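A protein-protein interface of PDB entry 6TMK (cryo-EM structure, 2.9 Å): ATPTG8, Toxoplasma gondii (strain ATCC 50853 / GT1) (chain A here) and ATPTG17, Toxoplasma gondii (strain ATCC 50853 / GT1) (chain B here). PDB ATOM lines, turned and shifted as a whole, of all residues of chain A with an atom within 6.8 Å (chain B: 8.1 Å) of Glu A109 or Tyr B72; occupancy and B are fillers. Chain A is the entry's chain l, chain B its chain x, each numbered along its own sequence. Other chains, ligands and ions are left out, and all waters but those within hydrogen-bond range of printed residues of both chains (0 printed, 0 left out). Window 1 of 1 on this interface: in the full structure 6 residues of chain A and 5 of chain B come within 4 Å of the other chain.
Printed residues of chain A that touch a printed residue of chain B: Val A105, Asp A106, Glu A109, Met A110, Asp A113 and Arg A141. Hydrophobic or aromatic side chains of chain A within 4 Å of the printed part of chain B: Val A105 and Met A110. Hydrophobic or aromatic side chains of chain B that line the printed part of chain A: Tyr B72 and His B74. Among the printed residues, 11 pairs touch across the chains. Among the printed residues, Asp or Glu carboxylates within 4 Å of a Lys or Arg side-chain nitrogen of the other chain: Glu A109 with Lys B71.
Of chain B, only Lys B71 and Tyr B72 come within 4 Å of Glu A109. Of chain A, only Asp A106 (2.7 Å), Glu A109 (3.2 Å), Met A110 (3.6 Å) and Asp A113 (2.7 Å) come within 4 Å of Tyr B72. Printed residues of chain B within 4 Å of Arg A141: Lys B71. Of the printed residues of chain A, Gly B75 touches Asp A106 (3.6 Å). Of the printed residues of chain A, His B74 touches Val A105 (3.7 Å) and Asp A106 (3.3 Å). The nearest residue of chain B that does not touch Glu A109 is Asn B73 (5.5 Å). The nearest residue of chain A that does not touch Tyr B72 is Ala A107 (5.8 Å).
Among the printed residues, merely in contact across the chains: Glu A109 with Tyr B72 (3.2 Å), Asp A106 with Asn B73 (3.5 Å), Met A110 with Tyr B72 (3.6 Å), Asp A106 with Gly B75 (3.6 Å), Val A105 with His B74 (3.7 Å), Arg A141 with Lys B71 (3.7 Å) and Asp A113 with Lys B71 (3.8 Å).
The backbone carbonyl oxygen (O) of Tyr B72 sits close to the side-chain carboxylate (OD2) of Asp A106 (2.7 Å). The backbone NH (N) of His B74 is in hydrogen-bond range of the side-chain carboxylate (OD1) of Asp A106, 3.3 Å away. The side-chain amino group of Lys B71 is in salt-bridge range of the side-chain carboxylate of Glu A109 (3.3 Å). OH of Tyr B72 sits at hydrogen-bond distance from OD2 of Asp A113 (2.7 Å).
The side-chain carboxylate of Asp A113 is in salt-bridge range of the guanidinium group of Arg A141 (3.8 Å). The side-chain carboxylate of Glu A116 lies within salt-bridge range of the guanidinium group of Arg A141, 3.7 Å away. ND2 of Asn B73 is in hydrogen-bond range of O of Glu B61 (2.5 Å). NZ of Lys B62 sits at hydrogen-bond distance from O of Asn B73.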
ATOM      1  N   VAL A  99      18.988 -16.403   0.437  1.00  0.00           N
ATOM      2  CA  VAL A  99      18.444 -16.226  -0.902  1.00  0.00           C
ATOM      3  C   VAL A  99      19.579 -16.351  -1.904  1.00  0.00           C
ATOM      4  O   VAL A  99      20.690 -15.860  -1.674  1.00  0.00           O
ATOM      5  CB  VAL A  99      17.730 -14.870  -1.034  1.00  0.00           C
ATOM      6  CG1 VAL A  99      16.611 -14.766  -0.031  1.00  0.00           C
ATOM      7  CG2 VAL A  99      18.706 -13.730  -0.856  1.00  0.00           C
ATOM      8  N   SER A 104      15.647 -13.565  -9.176  1.00  0.00           N
ATOM      9  CA  SER A 104      15.324 -12.156  -9.304  1.00  0.00           C
ATOM     10  C   SER A 104      14.872 -11.593  -7.963  1.00  0.00           C
ATOM     11  O   SER A 104      14.429 -12.320  -7.072  1.00  0.00           O
ATOM     12  CB  SER A 104      14.232 -11.949 -10.349  1.00  0.00           C
ATOM     13  OG  SER A 104      12.977 -12.384  -9.864  1.00  0.00           O
ATOM     14  N   VAL A 105      14.989 -10.273  -7.830  1.00  0.00           N
ATOM     15  CA  VAL A 105      14.745  -9.627  -6.543  1.00  0.00           C
ATOM     16  C   VAL A 105      13.317  -9.875  -6.074  1.00  0.00           C
ATOM     17  O   VAL A 105      13.061 -10.030  -4.872  1.00  0.00           O
ATOM     18  CB  VAL A 105      15.053  -8.125  -6.647  1.00  0.00           C
ATOM     19  CG1 VAL A 105      14.567  -7.399  -5.415  1.00  0.00           C
ATOM     20  CG2 VAL A 105      16.538  -7.912  -6.846  1.00  0.00           C
ATOM     21  N   ASP A 106      12.368  -9.930  -7.007  1.00  0.00           N
ATOM     22  CA  ASP A 106      10.990 -10.233  -6.635  1.00  0.00           C
ATOM     23  C   ASP A 106      10.877 -11.629  -6.041  1.00  0.00           C
ATOM     24  O   ASP A 106      10.197 -11.834  -5.028  1.00  0.00           O
ATOM     25  CB  ASP A 106      10.083 -10.095  -7.854  1.00  0.00           C
ATOM     26  CG  ASP A 106       9.836  -8.653  -8.234  1.00  0.00           C
ATOM     27  OD1 ASP A 106      10.274  -7.755  -7.486  1.00  0.00           O
ATOM     28  OD2 ASP A 106       9.203  -8.418  -9.286  1.00  0.00           O
ATOM     29  N   ALA A 107      11.553 -12.602  -6.649  1.00  0.00           N
ATOM     30  CA  ALA A 107      11.499 -13.962  -6.139  1.00  0.00           C
ATOM     31  C   ALA A 107      12.239 -14.085  -4.816  1.00  0.00           C
ATOM     32  O   ALA A 107      11.861 -14.899  -3.970  1.00  0.00           O
ATOM     33  CB  ALA A 107      12.077 -14.921  -7.171  1.00  0.00           C
ATOM     34  N   ARG A 108      13.290 -13.293  -4.621  1.00  0.00           N
ATOM     35  CA  ARG A 108      13.965 -13.258  -3.331  1.00  0.00           C
ATOM     36  C   ARG A 108      13.030 -12.735  -2.251  1.00  0.00           C
ATOM     37  O   ARG A 108      12.961 -13.284  -1.144  1.00  0.00           O
ATOM     38  CB  ARG A 108      15.208 -12.382  -3.425  1.00  0.00           C
ATOM     39  CG  ARG A 108      16.246 -12.873  -4.384  1.00  0.00           C
ATOM     40  CD  ARG A 108      17.397 -11.910  -4.449  1.00  0.00           C
ATOM     41  NE  ARG A 108      18.293 -12.184  -5.564  1.00  0.00           N
ATOM     42  CZ  ARG A 108      19.359 -11.450  -5.848  1.00  0.00           C
ATOM     43  NH1 ARG A 108      19.664 -10.406  -5.098  1.00  0.00           N
ATOM     44  NH2 ARG A 108      20.121 -11.764  -6.880  1.00  0.00           N
ATOM     45  N   GLU A 109      12.327 -11.644  -2.550  1.00  0.00           N
ATOM     46  CA  GLU A 109      11.319 -11.132  -1.633  1.00  0.00           C
ATOM     47  C   GLU A 109      10.283 -12.201  -1.312  1.00  0.00           C
ATOM     48  O   GLU A 109       9.891 -12.369  -0.152  1.00  0.00           O
ATOM     49  CB  GLU A 109      10.654  -9.902  -2.245  1.00  0.00           C
ATOM     50  CG  GLU A 109       9.784  -9.115  -1.296  1.00  0.00           C
ATOM     51  CD  GLU A 109       9.137  -7.920  -1.960  1.00  0.00           C
ATOM     52  OE1 GLU A 109       7.960  -7.636  -1.657  1.00  0.00           O
ATOM     53  OE2 GLU A 109       9.805  -7.267  -2.790  1.00  0.00           O
ATOM     54  N   MET A 110       9.838 -12.938  -2.328  1.00  0.00           N
ATOM     55  CA  MET A 110       8.848 -13.986  -2.107  1.00  0.00           C
ATOM     56  C   MET A 110       9.399 -15.090  -1.213  1.00  0.00           C
ATOM     57  O   MET A 110       8.702 -15.584  -0.320  1.00  0.00           O
ATOM     58  CB  MET A 110       8.397 -14.553  -3.450  1.00  0.00           C
ATOM     59  CG  MET A 110       7.379 -15.669  -3.366  1.00  0.00           C
ATOM     60  SD  MET A 110       5.949 -15.263  -2.363  1.00  0.00           S
ATOM     61  CE  MET A 110       5.046 -14.278  -3.539  1.00  0.00           C
ATOM     62  N   LYS A 111      10.647 -15.494  -1.445  1.00  0.00           N
ATOM     63  CA  LYS A 111      11.265 -16.526  -0.621  1.00  0.00           C
ATOM     64  C   LYS A 111      11.363 -16.084   0.829  1.00  0.00           C
ATOM     65  O   LYS A 111      11.080 -16.862   1.747  1.00  0.00           O
ATOM     66  CB  LYS A 111      12.650 -16.860  -1.165  1.00  0.00           C
ATOM     67  CG  LYS A 111      13.194 -18.193  -0.721  1.00  0.00           C
ATOM     68  CD  LYS A 111      14.554 -18.454  -1.301  1.00  0.00           C
ATOM     69  CE  LYS A 111      15.164 -19.707  -0.721  1.00  0.00           C
ATOM     70  NZ  LYS A 111      16.428 -20.096  -1.396  1.00  0.00           N
ATOM     71  N   VAL A 112      11.772 -14.836   1.056  1.00  0.00           N
ATOM     72  CA  VAL A 112      11.891 -14.342   2.419  1.00  0.00           C
ATOM     73  C   VAL A 112      10.522 -14.254   3.078  1.00  0.00           C
ATOM     74  O   VAL A 112      10.374 -14.540   4.271  1.00  0.00           O
ATOM     75  CB  VAL A 112      12.617 -12.989   2.429  1.00  0.00           C
ATOM     76  CG1 VAL A 112      12.590 -12.392   3.801  1.00  0.00           C
ATOM     77  CG2 VAL A 112      14.038 -13.170   1.984  1.00  0.00           C
ATOM     78  N   ASP A 113       9.498 -13.874   2.314  1.00  0.00           N
ATOM     79  CA  ASP A 113       8.151 -13.834   2.866  1.00  0.00           C
ATOM     80  C   ASP A 113       7.677 -15.228   3.247  1.00  0.00           C
ATOM     81  O   ASP A 113       7.013 -15.410   4.274  1.00  0.00           O
ATOM     82  CB  ASP A 113       7.191 -13.200   1.864  1.00  0.00           C
ATOM     83  CG  ASP A 113       7.436 -11.720   1.673  1.00  0.00           C
ATOM     84  OD1 ASP A 113       8.090 -11.105   2.541  1.00  0.00           O
ATOM     85  OD2 ASP A 113       6.967 -11.167   0.657  1.00  0.00           O
ATOM     86  N   MET A 114       8.005 -16.225   2.427  1.00  0.00           N
ATOM     87  CA  MET A 114       7.652 -17.603   2.747  1.00  0.00           C
ATOM     88  C   MET A 114       8.344 -18.064   4.021  1.00  0.00           C
ATOM     89  O   MET A 114       7.725 -18.680   4.898  1.00  0.00           O
ATOM     90  CB  MET A 114       8.034 -18.503   1.582  1.00  0.00           C
ATOM     91  CG  MET A 114       7.200 -18.284   0.348  1.00  0.00           C
ATOM     92  SD  MET A 114       8.148 -18.500  -1.162  1.00  0.00           S
ATOM     93  CE  MET A 114       7.892 -20.238  -1.439  1.00  0.00           C
ATOM     94  N   GLU A 116       9.383 -16.181   6.471  1.00  0.00           N
ATOM     95  CA  GLU A 116       8.818 -15.473   7.613  1.00  0.00           C
ATOM     96  C   GLU A 116       7.457 -16.033   7.992  1.00  0.00           C
ATOM     97  O   GLU A 116       7.171 -16.229   9.177  1.00  0.00           O
ATOM     98  CB  GLU A 116       8.711 -13.987   7.288  1.00  0.00           C
ATOM     99  CG  GLU A 116      10.049 -13.290   7.198  1.00  0.00           C
ATOM    100  CD  GLU A 116       9.940 -11.860   6.711  1.00  0.00           C
ATOM    101  OE1 GLU A 116       9.010 -11.564   5.932  1.00  0.00           O
ATOM    102  OE2 GLU A 116      10.791 -11.032   7.101  1.00  0.00           O
ATOM    103  N   ARG A 141      15.767  -9.238   4.385  1.00  0.00           N
ATOM    104  CA  ARG A 141      14.952  -8.261   3.671  1.00  0.00           C
ATOM    105  C   ARG A 141      15.726  -6.974   3.436  1.00  0.00           C
ATOM    106  O   ARG A 141      15.624  -6.360   2.368  1.00  0.00           O
ATOM    107  CB  ARG A 141      13.673  -7.960   4.445  1.00  0.00           C
ATOM    108  CG  ARG A 141      12.661  -9.069   4.434  1.00  0.00           C
ATOM    109  CD  ARG A 141      11.350  -8.604   5.038  1.00  0.00           C
ATOM    110  NE  ARG A 141      10.598  -7.790   4.094  1.00  0.00           N
ATOM    111  CZ  ARG A 141       9.879  -8.282   3.091  1.00  0.00           C
ATOM    112  NH1 ARG A 141       9.807  -9.589   2.903  1.00  0.00           N
ATOM    113  NH2 ARG A 141       9.232  -7.466   2.275  1.00  0.00           N
ATOM    114  N   LEU A 144      18.411  -7.832   0.471  1.00  0.00           N
ATOM    115  CA  LEU A 144      17.996  -8.588  -0.707  1.00  0.00           C
ATOM    116  C   LEU A 144      18.850  -8.245  -1.919  1.00  0.00           C
ATOM    117  O   LEU A 144      19.319  -9.137  -2.636  1.00  0.00           O
ATOM    118  CB  LEU A 144      16.528  -8.311  -1.014  1.00  0.00           C
ATOM    119  CG  LEU A 144      15.479  -8.964  -0.127  1.00  0.00           C
ATOM    120  CD1 LEU A 144      14.104  -8.608  -0.629  1.00  0.00           C
ATOM    121  CD2 LEU A 144      15.657 -10.457  -0.098  1.00  0.00           C
ATOM    122  N   GLU B  61       2.587   3.128 -11.525  1.00  0.00           N
ATOM    123  CA  GLU B  61       3.504   2.014 -11.720  1.00  0.00           C
ATOM    124  C   GLU B  61       4.180   1.602 -10.419  1.00  0.00           C
ATOM    125  O   GLU B  61       4.540   0.431 -10.255  1.00  0.00           O
ATOM    126  CB  GLU B  61       4.554   2.380 -12.764  1.00  0.00           C
ATOM    127  CG  GLU B  61       4.008   2.491 -14.170  1.00  0.00           C
ATOM    128  CD  GLU B  61       3.403   3.848 -14.455  1.00  0.00           C
ATOM    129  OE1 GLU B  61       3.101   4.579 -13.490  1.00  0.00           O
ATOM    130  OE2 GLU B  61       3.228   4.184 -15.644  1.00  0.00           O
ATOM    131  N   LYS B  62       4.359   2.539  -9.492  1.00  0.00           N
ATOM    132  CA  LYS B  62       5.091   2.302  -8.256  1.00  0.00           C
ATOM    133  C   LYS B  62       4.201   2.362  -7.023  1.00  0.00           C
ATOM    134  O   LYS B  62       4.716   2.345  -5.901  1.00  0.00           O
ATOM    135  CB  LYS B  62       6.229   3.315  -8.122  1.00  0.00           C
ATOM    136  CG  LYS B  62       7.292   3.229  -9.205  1.00  0.00           C
ATOM    137  CD  LYS B  62       8.264   2.089  -8.947  1.00  0.00           C
ATOM    138  CE  LYS B  62       8.932   1.606 -10.225  1.00  0.00           C
ATOM    139  NZ  LYS B  62       9.323   0.169 -10.145  1.00  0.00           N
ATOM    140  N   PRO B  69       3.422   1.238  -1.635  1.00  0.00           N
ATOM    141  CA  PRO B  69       4.243   0.751  -2.745  1.00  0.00           C
ATOM    142  C   PRO B  69       3.833  -0.641  -3.190  1.00  0.00           C
ATOM    143  O   PRO B  69       3.398  -1.474  -2.393  1.00  0.00           O
ATOM    144  CB  PRO B  69       5.660   0.753  -2.165  1.00  0.00           C
ATOM    145  CG  PRO B  69       5.595   1.696  -1.029  1.00  0.00           C
ATOM    146  CD  PRO B  69       4.243   1.521  -0.451  1.00  0.00           C
ATOM    147  N   ARG B  70       3.985  -0.886  -4.484  1.00  0.00           N
ATOM    148  CA  ARG B  70       3.628  -2.181  -5.041  1.00  0.00           C
ATOM    149  C   ARG B  70       4.644  -3.235  -4.632  1.00  0.00           C
ATOM    150  O   ARG B  70       5.856  -3.007  -4.692  1.00  0.00           O
ATOM    151  CB  ARG B  70       3.542  -2.095  -6.559  1.00  0.00           C
ATOM    152  CG  ARG B  70       2.243  -1.549  -7.068  1.00  0.00           C
ATOM    153  CD  ARG B  70       2.202  -1.548  -8.572  1.00  0.00           C
ATOM    154  NE  ARG B  70       1.176  -0.660  -9.100  1.00  0.00           N
ATOM    155  CZ  ARG B  70      -0.117  -0.949  -9.133  1.00  0.00           C
ATOM    156  NH1 ARG B  70      -0.562  -2.101  -8.671  1.00  0.00           N
ATOM    157  NH2 ARG B  70      -0.971  -0.079  -9.633  1.00  0.00           N
ATOM    158  N   LYS B  71       4.146  -4.390  -4.210  1.00  0.00           N
ATOM    159  CA  LYS B  71       5.004  -5.520  -3.890  1.00  0.00           C
ATOM    160  C   LYS B  71       5.438  -6.240  -5.158  1.00  0.00           C
ATOM    161  O   LYS B  71       4.658  -6.395  -6.100  1.00  0.00           O
ATOM    162  CB  LYS B  71       4.287  -6.492  -2.958  1.00  0.00           C
ATOM    163  CG  LYS B  71       4.285  -6.063  -1.513  1.00  0.00           C
ATOM    164  CD  LYS B  71       3.772  -7.161  -0.615  1.00  0.00           C
ATOM    165  CE  LYS B  71       4.906  -8.028  -0.128  1.00  0.00           C
ATOM    166  NZ  LYS B  71       5.767  -7.318   0.851  1.00  0.00           N
ATOM    167  N   TYR B  72       6.693  -6.685  -5.176  1.00  0.00           N
ATOM    168  CA  TYR B  72       7.224  -7.472  -6.286  1.00  0.00           C
ATOM    169  C   TYR B  72       7.218  -6.676  -7.587  1.00  0.00           C
ATOM    170  O   TYR B  72       6.854  -7.186  -8.647  1.00  0.00           O
ATOM    171  CB  TYR B  72       6.435  -8.770  -6.446  1.00  0.00           C
ATOM    172  CG  TYR B  72       6.150  -9.462  -5.140  1.00  0.00           C
ATOM    173  CD1 TYR B  72       7.152  -9.670  -4.213  1.00  0.00           C
ATOM    174  CD2 TYR B  72       4.878  -9.905  -4.835  1.00  0.00           C
ATOM    175  CE1 TYR B  72       6.894 -10.297  -3.019  1.00  0.00           C
ATOM    176  CE2 TYR B  72       4.612 -10.532  -3.646  1.00  0.00           C
ATOM    177  CZ  TYR B  72       5.624 -10.728  -2.742  1.00  0.00           C
ATOM    178  OH  TYR B  72       5.373 -11.354  -1.545  1.00  0.00           O
ATOM    179  N   ASN B  73       7.630  -5.412  -7.504  1.00  0.00           N
ATOM    180  CA  ASN B  73       7.618  -4.503  -8.642  1.00  0.00           C
ATOM    181  C   ASN B  73       9.014  -4.037  -9.035  1.00  0.00           C
ATOM    182  O   ASN B  73       9.140  -3.093  -9.821  1.00  0.00           O
ATOM    183  CB  ASN B  73       6.733  -3.295  -8.337  1.00  0.00           C
ATOM    184  CG  ASN B  73       6.127  -2.690  -9.578  1.00  0.00           C
ATOM    185  OD1 ASN B  73       5.618  -3.400 -10.444  1.00  0.00           O
ATOM    186  ND2 ASN B  73       6.178  -1.371  -9.674  1.00  0.00           N
ATOM    187  N   HIS B  74      10.063  -4.675  -8.520  1.00  0.00           N
ATOM    188  CA  HIS B  74      11.422  -4.236  -8.811  1.00  0.00           C
ATOM    189  C   HIS B  74      11.889  -4.721 -10.176  1.00  0.00           C
ATOM    190  O   HIS B  74      12.594  -3.995 -10.886  1.00  0.00           O
ATOM    191  CB  HIS B  74      12.371  -4.733  -7.721  1.00  0.00           C
ATOM    192  CG  HIS B  74      13.792  -4.306  -7.914  1.00  0.00           C
ATOM    193  ND1 HIS B  74      14.681  -5.009  -8.696  1.00  0.00           N
ATOM    194  CD2 HIS B  74      14.483  -3.255  -7.412  1.00  0.00           C
ATOM    195  CE1 HIS B  74      15.856  -4.405  -8.676  1.00  0.00           C
ATOM    196  NE2 HIS B  74      15.762  -3.338  -7.905  1.00  0.00           N
ATOM    197  N   GLY B  75      11.508  -5.936 -10.561  1.00  0.00           N
ATOM    198  CA  GLY B  75      11.911  -6.509 -11.824  1.00  0.00           C
ATOM    199  C   GLY B  75      10.863  -6.316 -12.905  1.00  0.00           C
ATOM    200  O   GLY B  75       9.855  -5.629 -12.730  1.00  0.00           O
ATOM    201  N   GLU B  76      11.121  -6.940 -14.050  1.00  0.00           N
ATOM    202  CA  GLU B  76      10.219  -6.902 -15.187  1.00  0.00           C
ATOM    203  C   GLU B  76       9.647  -8.286 -15.453  1.00  0.00           C
ATOM    204  O   GLU B  76      10.259  -9.305 -15.119  1.00  0.00           O
ATOM    205  CB  GLU B  76      10.936  -6.390 -16.433  1.00  0.00           C
ATOM    206  CG  GLU B  76      10.016  -5.748 -17.440  1.00  0.00           C
ATOM    207  CD  GLU B  76       9.474  -4.416 -16.960  1.00  0.00           C
ATOM    208  OE1 GLU B  76       8.571  -3.864 -17.623  1.00  0.00           O
ATOM    209  OE2 GLU B  76       9.950  -3.924 -15.917  1.00  0.00           O
ATOM    210  N   TRP B  77       8.463  -8.313 -16.058  1.00  0.00           N
ATOM    211  CA  TRP B  77       7.684  -9.533 -16.197  1.00  0.00           C
ATOM    212  C   TRP B  77       7.310  -9.748 -17.655  1.00  0.00           C
ATOM    213  O   TRP B  77       7.022  -8.794 -18.381  1.00  0.00           O
ATOM    214  CB  TRP B  77       6.433  -9.461 -15.327  1.00  0.00           C
ATOM    215  CG  TRP B  77       5.682 -10.732 -15.222  1.00  0.00           C
ATOM    216  CD1 TRP B  77       6.196 -11.986 -15.163  1.00  0.00           C
ATOM    217  CD2 TRP B  77       4.266 -10.876 -15.145  1.00  0.00           C
ATOM    218  NE1 TRP B  77       5.187 -12.907 -15.061  1.00  0.00           N
ATOM    219  CE2 TRP B  77       3.990 -12.246 -15.048  1.00  0.00           C
ATOM    220  CE3 TRP B  77       3.203  -9.976 -15.152  1.00  0.00           C
ATOM    221  CZ2 TRP B  77       2.699 -12.736 -14.959  1.00  0.00           C
ATOM    222  CZ3 TRP B  77       1.928 -10.465 -15.065  1.00  0.00           C
ATOM    223  CH2 TRP B  77       1.684 -11.830 -14.969  1.00  0.00           C
ATOM    224  N   SER B  82       2.121  -6.037 -13.888  1.00  0.00           N
ATOM    225  CA  SER B  82       1.679  -7.018 -12.914  1.00  0.00           C
ATOM    226  C   SER B  82       0.239  -6.810 -12.488  1.00  0.00           C
ATOM    227  O   SER B  82      -0.158  -7.281 -11.418  1.00  0.00           O
ATOM    228  CB  SER B  82       2.594  -6.960 -11.697  1.00  0.00           C
ATOM    229  OG  SER B  82       3.951  -6.975 -12.091  1.00  0.00           O
